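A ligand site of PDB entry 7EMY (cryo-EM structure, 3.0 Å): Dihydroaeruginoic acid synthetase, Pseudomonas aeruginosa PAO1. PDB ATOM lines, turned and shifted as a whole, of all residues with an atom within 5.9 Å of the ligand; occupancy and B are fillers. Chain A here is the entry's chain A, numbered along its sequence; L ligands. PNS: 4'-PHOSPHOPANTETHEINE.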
ATOM      1  N   ASP A  45     -19.043 -35.778  24.164  1.00  0.00           N
ATOM      2  CA  ASP A  45     -19.913 -34.615  24.011  1.00  0.00           C
ATOM      3  C   ASP A  45     -20.309 -34.441  22.544  1.00  0.00           C
ATOM      4  O   ASP A  45     -19.870 -35.195  21.671  1.00  0.00           O
ATOM      5  CB  ASP A  45     -19.260 -33.367  24.616  1.00  0.00           C
ATOM      6  CG  ASP A  45     -18.013 -32.880  23.877  1.00  0.00           C
ATOM      7  OD1 ASP A  45     -17.909 -33.078  22.653  1.00  0.00           O
ATOM      8  OD2 ASP A  45     -17.133 -32.279  24.524  1.00  0.00           O
ATOM      9  N   SER A  46     -21.150 -33.469  22.255  1.00  0.00           N
ATOM     10  CA  SER A  46     -21.655 -33.281  20.902  1.00  0.00           C
ATOM     11  C   SER A  46     -20.584 -32.781  19.952  1.00  0.00           C
ATOM     12  O   SER A  46     -20.673 -33.040  18.762  1.00  0.00           O
ATOM     13  CB  SER A  46     -22.753 -32.249  20.927  1.00  0.00           C
ATOM     14  OG  SER A  46     -23.624 -32.544  21.995  1.00  0.00           O
ATOM     15  N   ILE A  47     -19.565 -32.073  20.430  1.00  0.00           N
ATOM     16  CA  ILE A  47     -18.475 -31.596  19.591  1.00  0.00           C
ATOM     17  C   ILE A  47     -17.703 -32.803  19.082  1.00  0.00           C
ATOM     18  O   ILE A  47     -17.560 -32.995  17.870  1.00  0.00           O
ATOM     19  CB  ILE A  47     -17.588 -30.596  20.372  1.00  0.00           C
ATOM     20  CG1 ILE A  47     -18.369 -29.347  20.838  1.00  0.00           C
ATOM     21  CG2 ILE A  47     -16.412 -30.141  19.506  1.00  0.00           C
ATOM     22  CD1 ILE A  47     -19.123 -29.533  22.151  1.00  0.00           C
ATOM     23  N   MET A  50     -20.102 -34.971  16.771  1.00  0.00           N
ATOM     24  CA  MET A  50     -20.174 -34.414  15.425  1.00  0.00           C
ATOM     25  C   MET A  50     -18.874 -34.628  14.655  1.00  0.00           C
ATOM     26  O   MET A  50     -18.928 -34.926  13.460  1.00  0.00           O
ATOM     27  CB  MET A  50     -20.557 -32.938  15.436  1.00  0.00           C
ATOM     28  CG  MET A  50     -22.005 -32.671  15.844  1.00  0.00           C
ATOM     29  SD  MET A  50     -22.497 -30.941  15.797  1.00  0.00           S
ATOM     30  CE  MET A  50     -21.587 -30.313  17.214  1.00  0.00           C
ATOM     31  N   PHE A  65     -26.468 -37.515  13.256  1.00  0.00           N
ATOM     32  CA  PHE A  65     -26.081 -37.296  14.645  1.00  0.00           C
ATOM     33  C   PHE A  65     -27.217 -37.676  15.599  1.00  0.00           C
ATOM     34  O   PHE A  65     -26.947 -38.179  16.685  1.00  0.00           O
ATOM     35  CB  PHE A  65     -25.685 -35.831  14.826  1.00  0.00           C
ATOM     36  CG  PHE A  65     -25.261 -35.471  16.228  1.00  0.00           C
ATOM     37  CD1 PHE A  65     -26.240 -35.144  17.170  1.00  0.00           C
ATOM     38  CD2 PHE A  65     -23.906 -35.424  16.563  1.00  0.00           C
ATOM     39  CE1 PHE A  65     -25.844 -34.779  18.454  1.00  0.00           C
ATOM     40  CE2 PHE A  65     -23.522 -35.040  17.859  1.00  0.00           C
ATOM     41  CZ  PHE A  65     -24.496 -34.727  18.801  1.00  0.00           C
ATOM     42  N   TYR A 114     -25.745 -12.413  11.897  1.00  0.00           N
ATOM     43  CA  TYR A 114     -24.954 -11.432  12.637  1.00  0.00           C
ATOM     44  C   TYR A 114     -24.758 -10.136  11.848  1.00  0.00           C
ATOM     45  O   TYR A 114     -24.769  -9.053  12.416  1.00  0.00           O
ATOM     46  CB  TYR A 114     -23.603 -12.053  12.970  1.00  0.00           C
ATOM     47  CG  TYR A 114     -23.588 -13.244  13.903  1.00  0.00           C
ATOM     48  CD1 TYR A 114     -24.711 -13.628  14.670  1.00  0.00           C
ATOM     49  CD2 TYR A 114     -22.386 -13.963  14.039  1.00  0.00           C
ATOM     50  CE1 TYR A 114     -24.613 -14.693  15.587  1.00  0.00           C
ATOM     51  CE2 TYR A 114     -22.287 -15.005  14.964  1.00  0.00           C
ATOM     52  CZ  TYR A 114     -23.398 -15.369  15.748  1.00  0.00           C
ATOM     53  OH  TYR A 114     -23.313 -16.386  16.644  1.00  0.00           O
ATOM     54  N   LEU A 236     -17.682 -11.747  15.950  1.00  0.00           N
ATOM     55  CA  LEU A 236     -17.914 -13.139  15.659  1.00  0.00           C
ATOM     56  C   LEU A 236     -18.335 -13.386  14.208  1.00  0.00           C
ATOM     57  O   LEU A 236     -18.258 -14.521  13.783  1.00  0.00           O
ATOM     58  CB  LEU A 236     -18.856 -13.803  16.656  1.00  0.00           C
ATOM     59  CG  LEU A 236     -18.399 -13.806  18.118  1.00  0.00           C
ATOM     60  CD1 LEU A 236     -18.925 -15.097  18.738  1.00  0.00           C
ATOM     61  CD2 LEU A 236     -16.889 -13.787  18.383  1.00  0.00           C
ATOM     62  N   ASP A 240     -15.737 -17.922  15.064  1.00  0.00           N
ATOM     63  CA  ASP A 240     -16.484 -18.728  16.031  1.00  0.00           C
ATOM     64  C   ASP A 240     -15.839 -18.485  17.417  1.00  0.00           C
ATOM     65  O   ASP A 240     -14.704 -18.044  17.492  1.00  0.00           O
ATOM     66  CB  ASP A 240     -16.374 -20.174  15.510  1.00  0.00           C
ATOM     67  CG  ASP A 240     -16.990 -21.286  16.350  1.00  0.00           C
ATOM     68  OD1 ASP A 240     -17.355 -21.074  17.524  1.00  0.00           O
ATOM     69  OD2 ASP A 240     -16.989 -22.433  15.840  1.00  0.00           O
ATOM     70  N   VAL A 241     -16.491 -18.771  18.552  1.00  0.00           N
ATOM     71  CA  VAL A 241     -15.753 -18.668  19.827  1.00  0.00           C
ATOM     72  C   VAL A 241     -14.729 -19.778  19.997  1.00  0.00           C
ATOM     73  O   VAL A 241     -13.756 -19.609  20.728  1.00  0.00           O
ATOM     74  CB  VAL A 241     -16.619 -18.579  21.070  1.00  0.00           C
ATOM     75  CG1 VAL A 241     -17.643 -17.469  20.962  1.00  0.00           C
ATOM     76  CG2 VAL A 241     -17.279 -19.887  21.412  1.00  0.00           C
ATOM     77  N   GLU A 242     -14.870 -20.900  19.309  1.00  0.00           N
ATOM     78  CA  GLU A 242     -13.769 -21.863  19.237  1.00  0.00           C
ATOM     79  C   GLU A 242     -12.577 -21.231  18.479  1.00  0.00           C
ATOM     80  O   GLU A 242     -11.419 -21.276  18.850  1.00  0.00           O
ATOM     81  CB  GLU A 242     -14.290 -23.162  18.629  1.00  0.00           C
ATOM     82  CG  GLU A 242     -13.569 -24.370  19.236  1.00  0.00           C
ATOM     83  CD  GLU A 242     -12.074 -24.388  18.913  1.00  0.00           C
ATOM     84  OE1 GLU A 242     -11.761 -24.198  17.721  1.00  0.00           O
ATOM     85  OE2 GLU A 242     -11.279 -24.603  19.852  1.00  0.00           O
ATOM     86  N   THR A 343     -24.830 -35.404  27.675  1.00  0.00           N
ATOM     87  CA  THR A 343     -23.775 -34.422  27.491  1.00  0.00           C
ATOM     88  C   THR A 343     -23.930 -33.328  28.517  1.00  0.00           C
ATOM     89  O   THR A 343     -25.024 -32.930  28.895  1.00  0.00           O
ATOM     90  CB  THR A 343     -23.796 -33.772  26.108  1.00  0.00           C
ATOM     91  OG1 THR A 343     -25.011 -33.149  25.901  1.00  0.00           O
ATOM     92  CG2 THR A 343     -23.567 -34.803  25.001  1.00  0.00           C
ATOM     93  N   LEU A 344     -22.808 -32.793  28.977  1.00  0.00           N
ATOM     94  CA  LEU A 344     -22.812 -31.684  29.920  1.00  0.00           C
ATOM     95  C   LEU A 344     -23.488 -30.438  29.333  1.00  0.00           C
ATOM     96  O   LEU A 344     -24.185 -29.707  30.014  1.00  0.00           O
ATOM     97  CB  LEU A 344     -21.355 -31.422  30.291  1.00  0.00           C
ATOM     98  CG  LEU A 344     -21.220 -30.316  31.329  1.00  0.00           C
ATOM     99  CD1 LEU A 344     -21.800 -30.711  32.682  1.00  0.00           C
ATOM    100  CD2 LEU A 344     -19.755 -29.991  31.499  1.00  0.00           C
ATOM    101  N   SER A 345     -23.305 -30.204  28.041  1.00  0.00           N
ATOM    102  CA  SER A 345     -23.961 -29.109  27.347  1.00  0.00           C
ATOM    103  C   SER A 345     -25.476 -29.279  27.360  1.00  0.00           C
ATOM    104  O   SER A 345     -26.170 -28.329  27.688  1.00  0.00           O
ATOM    105  CB  SER A 345     -23.460 -29.026  25.910  1.00  0.00           C
ATOM    106  OG  SER A 345     -22.175 -29.604  25.722  1.00  0.00           O
ATOM    107  N   SER A 346     -26.018 -30.479  27.149  1.00  0.00           N
ATOM    108  CA  SER A 346     -27.431 -30.726  27.392  1.00  0.00           C
ATOM    109  C   SER A 346     -27.850 -30.458  28.818  1.00  0.00           C
ATOM    110  O   SER A 346     -28.963 -29.992  29.020  1.00  0.00           O
ATOM    111  CB  SER A 346     -27.826 -32.167  27.086  1.00  0.00           C
ATOM    112  OG  SER A 346     -27.676 -32.455  25.726  1.00  0.00           O
ATOM    113  N   VAL A 369     -29.171 -22.180  19.482  1.00  0.00           N
ATOM    114  CA  VAL A 369     -27.995 -22.899  19.940  1.00  0.00           C
ATOM    115  C   VAL A 369     -26.969 -22.760  18.842  1.00  0.00           C
ATOM    116  O   VAL A 369     -27.097 -23.399  17.809  1.00  0.00           O
ATOM    117  CB  VAL A 369     -28.337 -24.352  20.248  1.00  0.00           C
ATOM    118  CG1 VAL A 369     -27.111 -25.068  20.798  1.00  0.00           C
ATOM    119  CG2 VAL A 369     -29.447 -24.438  21.298  1.00  0.00           C
ATOM    120  N   PRO A 370     -25.960 -21.898  18.942  1.00  0.00           N
ATOM    121  CA  PRO A 370     -24.863 -21.944  18.007  1.00  0.00           C
ATOM    122  C   PRO A 370     -24.186 -23.302  18.122  1.00  0.00           C
ATOM    123  O   PRO A 370     -23.626 -23.637  19.158  1.00  0.00           O
ATOM    124  CB  PRO A 370     -23.972 -20.770  18.365  1.00  0.00           C
ATOM    125  CG  PRO A 370     -24.336 -20.438  19.795  1.00  0.00           C
ATOM    126  CD  PRO A 370     -25.807 -20.809  19.865  1.00  0.00           C
ATOM    127  N   LEU A 371     -24.275 -24.107  17.073  1.00  0.00           N
ATOM    128  CA  LEU A 371     -23.524 -25.335  16.979  1.00  0.00           C
ATOM    129  C   LEU A 371     -22.120 -25.033  16.509  1.00  0.00           C
ATOM    130  O   LEU A 371     -21.900 -24.291  15.551  1.00  0.00           O
ATOM    131  CB  LEU A 371     -24.107 -26.335  15.984  1.00  0.00           C
ATOM    132  CG  LEU A 371     -25.598 -26.623  16.093  1.00  0.00           C
ATOM    133  CD1 LEU A 371     -25.922 -27.742  15.114  1.00  0.00           C
ATOM    134  CD2 LEU A 371     -25.955 -27.060  17.486  1.00  0.00           C
ATOM    135  N   PHE A 372     -21.187 -25.762  17.098  1.00  0.00           N
ATOM    136  CA  PHE A 372     -19.943 -26.085  16.450  1.00  0.00           C
ATOM    137  C   PHE A 372     -20.245 -26.770  15.119  1.00  0.00           C
ATOM    138  O   PHE A 372     -20.925 -27.786  15.085  1.00  0.00           O
ATOM    139  CB  PHE A 372     -19.184 -27.009  17.386  1.00  0.00           C
ATOM    140  CG  PHE A 372     -17.856 -27.512  16.897  1.00  0.00           C
ATOM    141  CD1 PHE A 372     -17.787 -28.681  16.119  1.00  0.00           C
ATOM    142  CD2 PHE A 372     -16.680 -26.868  17.297  1.00  0.00           C
ATOM    143  CE1 PHE A 372     -16.542 -29.212  15.762  1.00  0.00           C
ATOM    144  CE2 PHE A 372     -15.439 -27.417  16.962  1.00  0.00           C
ATOM    145  CZ  PHE A 372     -15.376 -28.580  16.195  1.00  0.00           C
ATOM    146  N   THR A 389     -19.354 -21.421  13.004  1.00  0.00           N
ATOM    147  CA  THR A 389     -20.590 -21.687  13.694  1.00  0.00           C
ATOM    148  C   THR A 389     -21.689 -21.961  12.658  1.00  0.00           C
ATOM    149  O   THR A 389     -21.655 -21.471  11.541  1.00  0.00           O
ATOM    150  CB  THR A 389     -20.941 -20.482  14.567  1.00  0.00           C
ATOM    151  OG1 THR A 389     -19.799 -19.903  15.153  1.00  0.00           O
ATOM    152  CG2 THR A 389     -21.920 -20.845  15.662  1.00  0.00           C
ATOM    153  N   LEU A 392     -28.490 -23.335  15.295  1.00  0.00           N
ATOM    154  CA  LEU A 392     -29.579 -24.285  15.452  1.00  0.00           C
ATOM    155  C   LEU A 392     -30.755 -23.608  16.132  1.00  0.00           C
ATOM    156  O   LEU A 392     -30.619 -23.094  17.244  1.00  0.00           O
ATOM    157  CB  LEU A 392     -29.099 -25.516  16.242  1.00  0.00           C
ATOM    158  CG  LEU A 392     -30.237 -26.302  16.899  1.00  0.00           C
ATOM    159  CD1 LEU A 392     -31.279 -26.818  15.910  1.00  0.00           C
ATOM    160  CD2 LEU A 392     -29.712 -27.503  17.667  1.00  0.00           C
ATOM    161  N   GLN A 412     -31.915 -33.269  25.746  1.00  0.00           N
ATOM    162  CA  GLN A 412     -30.817 -33.830  25.001  1.00  0.00           C
ATOM    163  C   GLN A 412     -31.332 -34.432  23.707  1.00  0.00           C
ATOM    164  O   GLN A 412     -30.863 -34.083  22.635  1.00  0.00           O
ATOM    165  CB  GLN A 412     -30.124 -34.882  25.857  1.00  0.00           C
ATOM    166  CG  GLN A 412     -29.194 -35.720  24.993  1.00  0.00           C
ATOM    167  CD  GLN A 412     -28.162 -36.459  25.799  1.00  0.00           C
ATOM    168  OE1 GLN A 412     -27.192 -35.880  26.235  1.00  0.00           O
ATOM    169  NE2 GLN A 412     -28.332 -37.739  26.019  1.00  0.00           N
ATOM    170  N   LEU A 415     -32.444 -31.761  21.273  1.00  0.00           N
ATOM    171  CA  LEU A 415     -31.276 -31.040  20.779  1.00  0.00           C
ATOM    172  C   LEU A 415     -30.539 -31.893  19.750  1.00  0.00           C
ATOM    173  O   LEU A 415     -30.251 -31.442  18.646  1.00  0.00           O
ATOM    174  CB  LEU A 415     -30.412 -30.661  21.988  1.00  0.00           C
ATOM    175  CG  LEU A 415     -29.000 -30.161  21.654  1.00  0.00           C
ATOM    176  CD1 LEU A 415     -29.004 -28.845  20.895  1.00  0.00           C
ATOM    177  CD2 LEU A 415     -28.217 -29.922  22.931  1.00  0.00           C
ATOM    178  N   HIS A 416     -30.269 -33.146  20.093  1.00  0.00           N
ATOM    179  CA  HIS A 416     -29.567 -34.056  19.229  1.00  0.00           C
ATOM    180  C   HIS A 416     -30.300 -34.322  17.924  1.00  0.00           C
ATOM    181  O   HIS A 416     -29.698 -34.323  16.871  1.00  0.00           O
ATOM    182  CB  HIS A 416     -29.306 -35.341  20.017  1.00  0.00           C
ATOM    183  CG  HIS A 416     -28.319 -35.212  21.147  1.00  0.00           C
ATOM    184  ND1 HIS A 416     -27.889 -36.251  21.943  1.00  0.00           N
ATOM    185  CD2 HIS A 416     -27.557 -34.128  21.476  1.00  0.00           C
ATOM    186  CE1 HIS A 416     -26.836 -35.822  22.650  1.00  0.00           C
ATOM    187  NE2 HIS A 416     -26.607 -34.529  22.407  1.00  0.00           N
ATOM    188  N   ILE A 419     -29.952 -31.193  15.775  1.00  0.00           N
ATOM    189  CA  ILE A 419     -28.592 -30.914  15.314  1.00  0.00           C
ATOM    190  C   ILE A 419     -28.423 -31.284  13.844  1.00  0.00           C
ATOM    191  O   ILE A 419     -27.871 -30.523  13.063  1.00  0.00           O
ATOM    192  CB  ILE A 419     -27.542 -31.586  16.234  1.00  0.00           C
ATOM    193  CG1 ILE A 419     -27.242 -30.655  17.426  1.00  0.00           C
ATOM    194  CG2 ILE A 419     -26.235 -31.940  15.514  1.00  0.00           C
ATOM    195  CD1 ILE A 419     -26.494 -31.291  18.588  1.00  0.00           C
ATOM    196  N   VAL A 445     -30.015 -17.105  23.202  1.00  0.00           N
ATOM    197  CA  VAL A 445     -28.931 -17.948  22.736  1.00  0.00           C
ATOM    198  C   VAL A 445     -28.447 -18.848  23.849  1.00  0.00           C
ATOM    199  O   VAL A 445     -28.401 -18.433  24.986  1.00  0.00           O
ATOM    200  CB  VAL A 445     -27.803 -17.106  22.119  1.00  0.00           C
ATOM    201  CG1 VAL A 445     -26.446 -17.785  22.056  1.00  0.00           C
ATOM    202  CG2 VAL A 445     -28.182 -16.731  20.695  1.00  0.00           C
ATOM    203  N   PHE A 446     -28.101 -20.084  23.511  1.00  0.00           N
ATOM    204  CA  PHE A 446     -27.395 -21.019  24.367  1.00  0.00           C
ATOM    205  C   PHE A 446     -26.131 -21.485  23.653  1.00  0.00           C
ATOM    206  O   PHE A 446     -26.107 -22.496  22.954  1.00  0.00           O
ATOM    207  CB  PHE A 446     -28.344 -22.151  24.754  1.00  0.00           C
ATOM    208  CG  PHE A 446     -27.672 -23.301  25.438  1.00  0.00           C
ATOM    209  CD1 PHE A 446     -27.115 -23.104  26.702  1.00  0.00           C
ATOM    210  CD2 PHE A 446     -27.527 -24.547  24.804  1.00  0.00           C
ATOM    211  CE1 PHE A 446     -26.398 -24.141  27.317  1.00  0.00           C
ATOM    212  CE2 PHE A 446     -26.762 -25.567  25.387  1.00  0.00           C
ATOM    213  CZ  PHE A 446     -26.182 -25.340  26.634  1.00  0.00           C
ATOM    214  N   ALA A 447     -25.066 -20.723  23.780  1.00  0.00           N
ATOM    215  CA  ALA A 447     -23.726 -21.117  23.373  1.00  0.00           C
ATOM    216  C   ALA A 447     -23.098 -21.989  24.455  1.00  0.00           C
ATOM    217  O   ALA A 447     -23.255 -21.698  25.622  1.00  0.00           O
ATOM    218  CB  ALA A 447     -22.910 -19.859  23.167  1.00  0.00           C
ATOM    219  N   SER A 448     -22.322 -23.015  24.106  1.00  0.00           N
ATOM    220  CA  SER A 448     -21.651 -23.805  25.132  1.00  0.00           C
ATOM    221  C   SER A 448     -20.331 -24.370  24.649  1.00  0.00           C
ATOM    222  O   SER A 448     -20.283 -25.134  23.693  1.00  0.00           O
ATOM    223  CB  SER A 448     -22.600 -24.869  25.658  1.00  0.00           C
ATOM    224  OG  SER A 448     -22.759 -25.937  24.775  1.00  0.00           O
ATOM    225  N   ASN A 449     -19.236 -23.972  25.288  1.00  0.00           N
ATOM    226  CA  ASN A 449     -17.891 -24.095  24.717  1.00  0.00           C
ATOM    227  C   ASN A 449     -17.039 -25.031  25.574  1.00  0.00           C
ATOM    228  O   ASN A 449     -15.987 -24.670  26.071  1.00  0.00           O
ATOM    229  CB  ASN A 449     -17.338 -22.689  24.523  1.00  0.00           C
ATOM    230  CG  ASN A 449     -18.370 -21.844  23.812  1.00  0.00           C
ATOM    231  OD1 ASN A 449     -18.770 -22.144  22.708  1.00  0.00           O
ATOM    232  ND2 ASN A 449     -18.898 -20.822  24.438  1.00  0.00           N
ATOM    233  N   THR A 474     -24.305 -10.179  20.710  1.00  0.00           N
ATOM    234  CA  THR A 474     -25.134 -10.793  19.665  1.00  0.00           C
ATOM    235  C   THR A 474     -26.387  -9.973  19.389  1.00  0.00           C
ATOM    236  O   THR A 474     -27.159  -9.724  20.315  1.00  0.00           O
ATOM    237  CB  THR A 474     -25.529 -12.233  19.962  1.00  0.00           C
ATOM    238  OG1 THR A 474     -24.406 -12.979  20.249  1.00  0.00           O
ATOM    239  CG2 THR A 474     -26.093 -12.905  18.714  1.00  0.00           C
ATOM    240  N   ASP A 480     -27.959 -13.738  25.639  1.00  0.00           N
ATOM    241  CA  ASP A 480     -26.917 -14.596  25.101  1.00  0.00           C
ATOM    242  C   ASP A 480     -26.243 -15.385  26.209  1.00  0.00           C
ATOM    243  O   ASP A 480     -25.323 -14.913  26.867  1.00  0.00           O
ATOM    244  CB  ASP A 480     -25.979 -13.738  24.245  1.00  0.00           C
ATOM    245  CG  ASP A 480     -24.915 -14.559  23.526  1.00  0.00           C
ATOM    246  OD1 ASP A 480     -24.708 -15.722  23.896  1.00  0.00           O
ATOM    247  OD2 ASP A 480     -24.318 -14.015  22.578  1.00  0.00           O
ATOM    248  N   GLN A 482     -23.868 -18.088  27.580  1.00  0.00           N
ATOM    249  CA  GLN A 482     -22.661 -18.753  27.189  1.00  0.00           C
ATOM    250  C   GLN A 482     -22.061 -19.485  28.359  1.00  0.00           C
ATOM    251  O   GLN A 482     -22.343 -19.170  29.518  1.00  0.00           O
ATOM    252  CB  GLN A 482     -21.660 -17.760  26.648  1.00  0.00           C
ATOM    253  CG  GLN A 482     -22.166 -16.891  25.491  1.00  0.00           C
ATOM    254  CD  GLN A 482     -21.699 -15.469  25.681  1.00  0.00           C
ATOM    255  OE1 GLN A 482     -20.520 -15.192  25.769  1.00  0.00           O
ATOM    256  NE2 GLN A 482     -22.586 -14.550  25.886  1.00  0.00           N
ATOM    257  N   TYR A 484     -18.163 -21.305  29.398  1.00  0.00           N
ATOM    258  CA  TYR A 484     -16.738 -21.347  29.132  1.00  0.00           C
ATOM    259  C   TYR A 484     -16.022 -22.129  30.200  1.00  0.00           C
ATOM    260  O   TYR A 484     -16.282 -21.955  31.375  1.00  0.00           O
ATOM    261  CB  TYR A 484     -16.190 -19.927  29.071  1.00  0.00           C
ATOM    262  CG  TYR A 484     -16.860 -19.085  28.031  1.00  0.00           C
ATOM    263  CD1 TYR A 484     -16.592 -19.368  26.688  1.00  0.00           C
ATOM    264  CD2 TYR A 484     -17.771 -18.084  28.388  1.00  0.00           C
ATOM    265  CE1 TYR A 484     -17.225 -18.647  25.689  1.00  0.00           C
ATOM    266  CE2 TYR A 484     -18.447 -17.378  27.380  1.00  0.00           C
ATOM    267  CZ  TYR A 484     -18.177 -17.676  26.027  1.00  0.00           C
ATOM    268  OH  TYR A 484     -18.892 -17.141  25.018  1.00  0.00           O
HETATM  269  O23 PNS L   1     -24.777 -31.452  24.083  1.00  0.00           O
HETATM  270  P24 PNS L   1     -23.701 -31.228  23.101  1.00  0.00           P
HETATM  271  O26 PNS L   1     -22.336 -31.252  23.705  1.00  0.00           O
HETATM  272  O27 PNS L   1     -23.921 -29.996  22.105  1.00  0.00           O
HETATM  273  C28 PNS L   1     -23.220 -28.755  22.210  1.00  0.00           C
HETATM  274  C29 PNS L   1     -23.636 -27.943  20.956  1.00  0.00           C
HETATM  275  C30 PNS L   1     -23.159 -28.693  19.686  1.00  0.00           C
HETATM  276  C31 PNS L   1     -25.176 -27.860  20.946  1.00  0.00           C
HETATM  277  C32 PNS L   1     -23.085 -26.478  20.912  1.00  0.00           C
HETATM  278  O33 PNS L   1     -23.531 -25.710  22.041  1.00  0.00           O
HETATM  279  C34 PNS L   1     -21.567 -26.322  20.684  1.00  0.00           C
HETATM  280  O35 PNS L   1     -20.760 -27.231  20.781  1.00  0.00           O
HETATM  281  N36 PNS L   1     -21.163 -25.051  20.336  1.00  0.00           N
HETATM  282  C37 PNS L   1     -19.788 -24.593  20.515  1.00  0.00           C
HETATM  283  C38 PNS L   1     -19.418 -23.507  19.501  1.00  0.00           C
HETATM  284  C39 PNS L   1     -20.240 -22.243  19.678  1.00  0.00           C
HETATM  285  O40 PNS L   1     -21.229 -22.198  20.377  1.00  0.00           O
HETATM  286  N41 PNS L   1     -19.775 -21.161  18.973  1.00  0.00           N
HETATM  287  C42 PNS L   1     -20.356 -19.813  18.922  1.00  0.00           C
HETATM  288  C43 PNS L   1     -20.888 -19.293  20.271  1.00  0.00           C
HETATM  289  S44 PNS L   1     -21.645 -17.640  20.018  1.00  0.00           S
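The side-chain hydroxyl (OG1) of Thr 343 lies within hydrogen-bond range of the side-chain hydroxyl (OG) of Ser 346, 2.8 Å away.
N of Thr 343 lies within hydrogen-bond range of OE1 of Gln 412 (2.8 Å).
The side-chain carboxylate (OD1) of Asp 240 lies within hydrogen-bond range of the backbone NH (N) of Glu 242 (3.1 Å).
N of Ile 47 lies within hydrogen-bond range of OD1 of Asp 45, 2.9 Å away.
The backbone carbonyl oxygen of Leu 392 sits at hydrogen-bond distance from the backbone NH of Val 369 (2.8 Å).
The side-chain amide oxygen (OE1) of Gln 412 sits close to the side-chain hydroxyl (OG) of Ser 346 (3.5 Å).
Residues that only touch the ligand: Asp 45 (3.8 Å), Ile 47 (3.1 Å), Met 50 (3.3 Å), Tyr 114 (3.97 Å), Leu 236 (3.9 Å), Val 241 (3.7 Å), Val 369 (3.4 Å), Leu 371 (3.6 Å), Thr 389 (3.8 Å), Leu 415 (3.9 Å), His 416 (3.95 Å) and Ala 447 (3.6 Å).
Hydrophobic or aromatic side chains within 4 Å of the ligand: Ile 47, Met 50, Leu 236, Val 241, Val 369, Pro 370, Leu 371, Phe 372, Leu 415 and Ala 447.
21 residues have an atom within 4 Å of the ligand: Asp 45, Ser 46, Ile 47, Met 50, Tyr 114, Leu 236, Asp 240, Val 241, Thr 343, Ser 345, Ser 346, Val 369, Pro 370, Leu 371, Phe 372, Thr 389, Leu 415, His 416, Ala 447, Ser 448 and Asn 449.
Along chain A the residues within 4 Å of the ligand span positions 45 to 449.
An oxygen (O26) of the ligand lies close to the backbone NH (N) of Ser 46 (2.9 Å).
The side-chain hydroxyl (OG) of Ser 46 is bonded to a phosphorus (P24) of the ligand (1.7 Å).
An oxygen (O23) of the ligand lies close to the side-chain hydroxyl of Thr 343, at 2.5 Å.
An oxygen (O26) of the ligand lies close to the side-chain hydroxyl (OG) of Ser 345 (2.6 Å).
OD1 of Asp 240 sits close to N41 of the ligand, 2.8 Å away.
O of Ser 448 sits close to N36 of the ligand (3.5 Å).
The side-chain hydroxyl of Ser 448 lies close to an oxygen (O33) of the ligand, at 2.8 Å.
The backbone carbonyl oxygen of Pro 370 sits close to an oxygen (O40) of the ligand (3.0 Å).
The backbone NH (N) of Phe 372 sits close to a nitrogen (N36) of the ligand (3.3 Å).
O40 of the ligand sits close to OD1 of Asn 449, 3.4 Å away.
An oxygen (O23) of the ligand sits close to the backbone NH of Ser 346.
An oxygen (O23) of the ligand sits close to the side-chain hydroxyl (OG) of Ser 346, 3.5 Å away.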
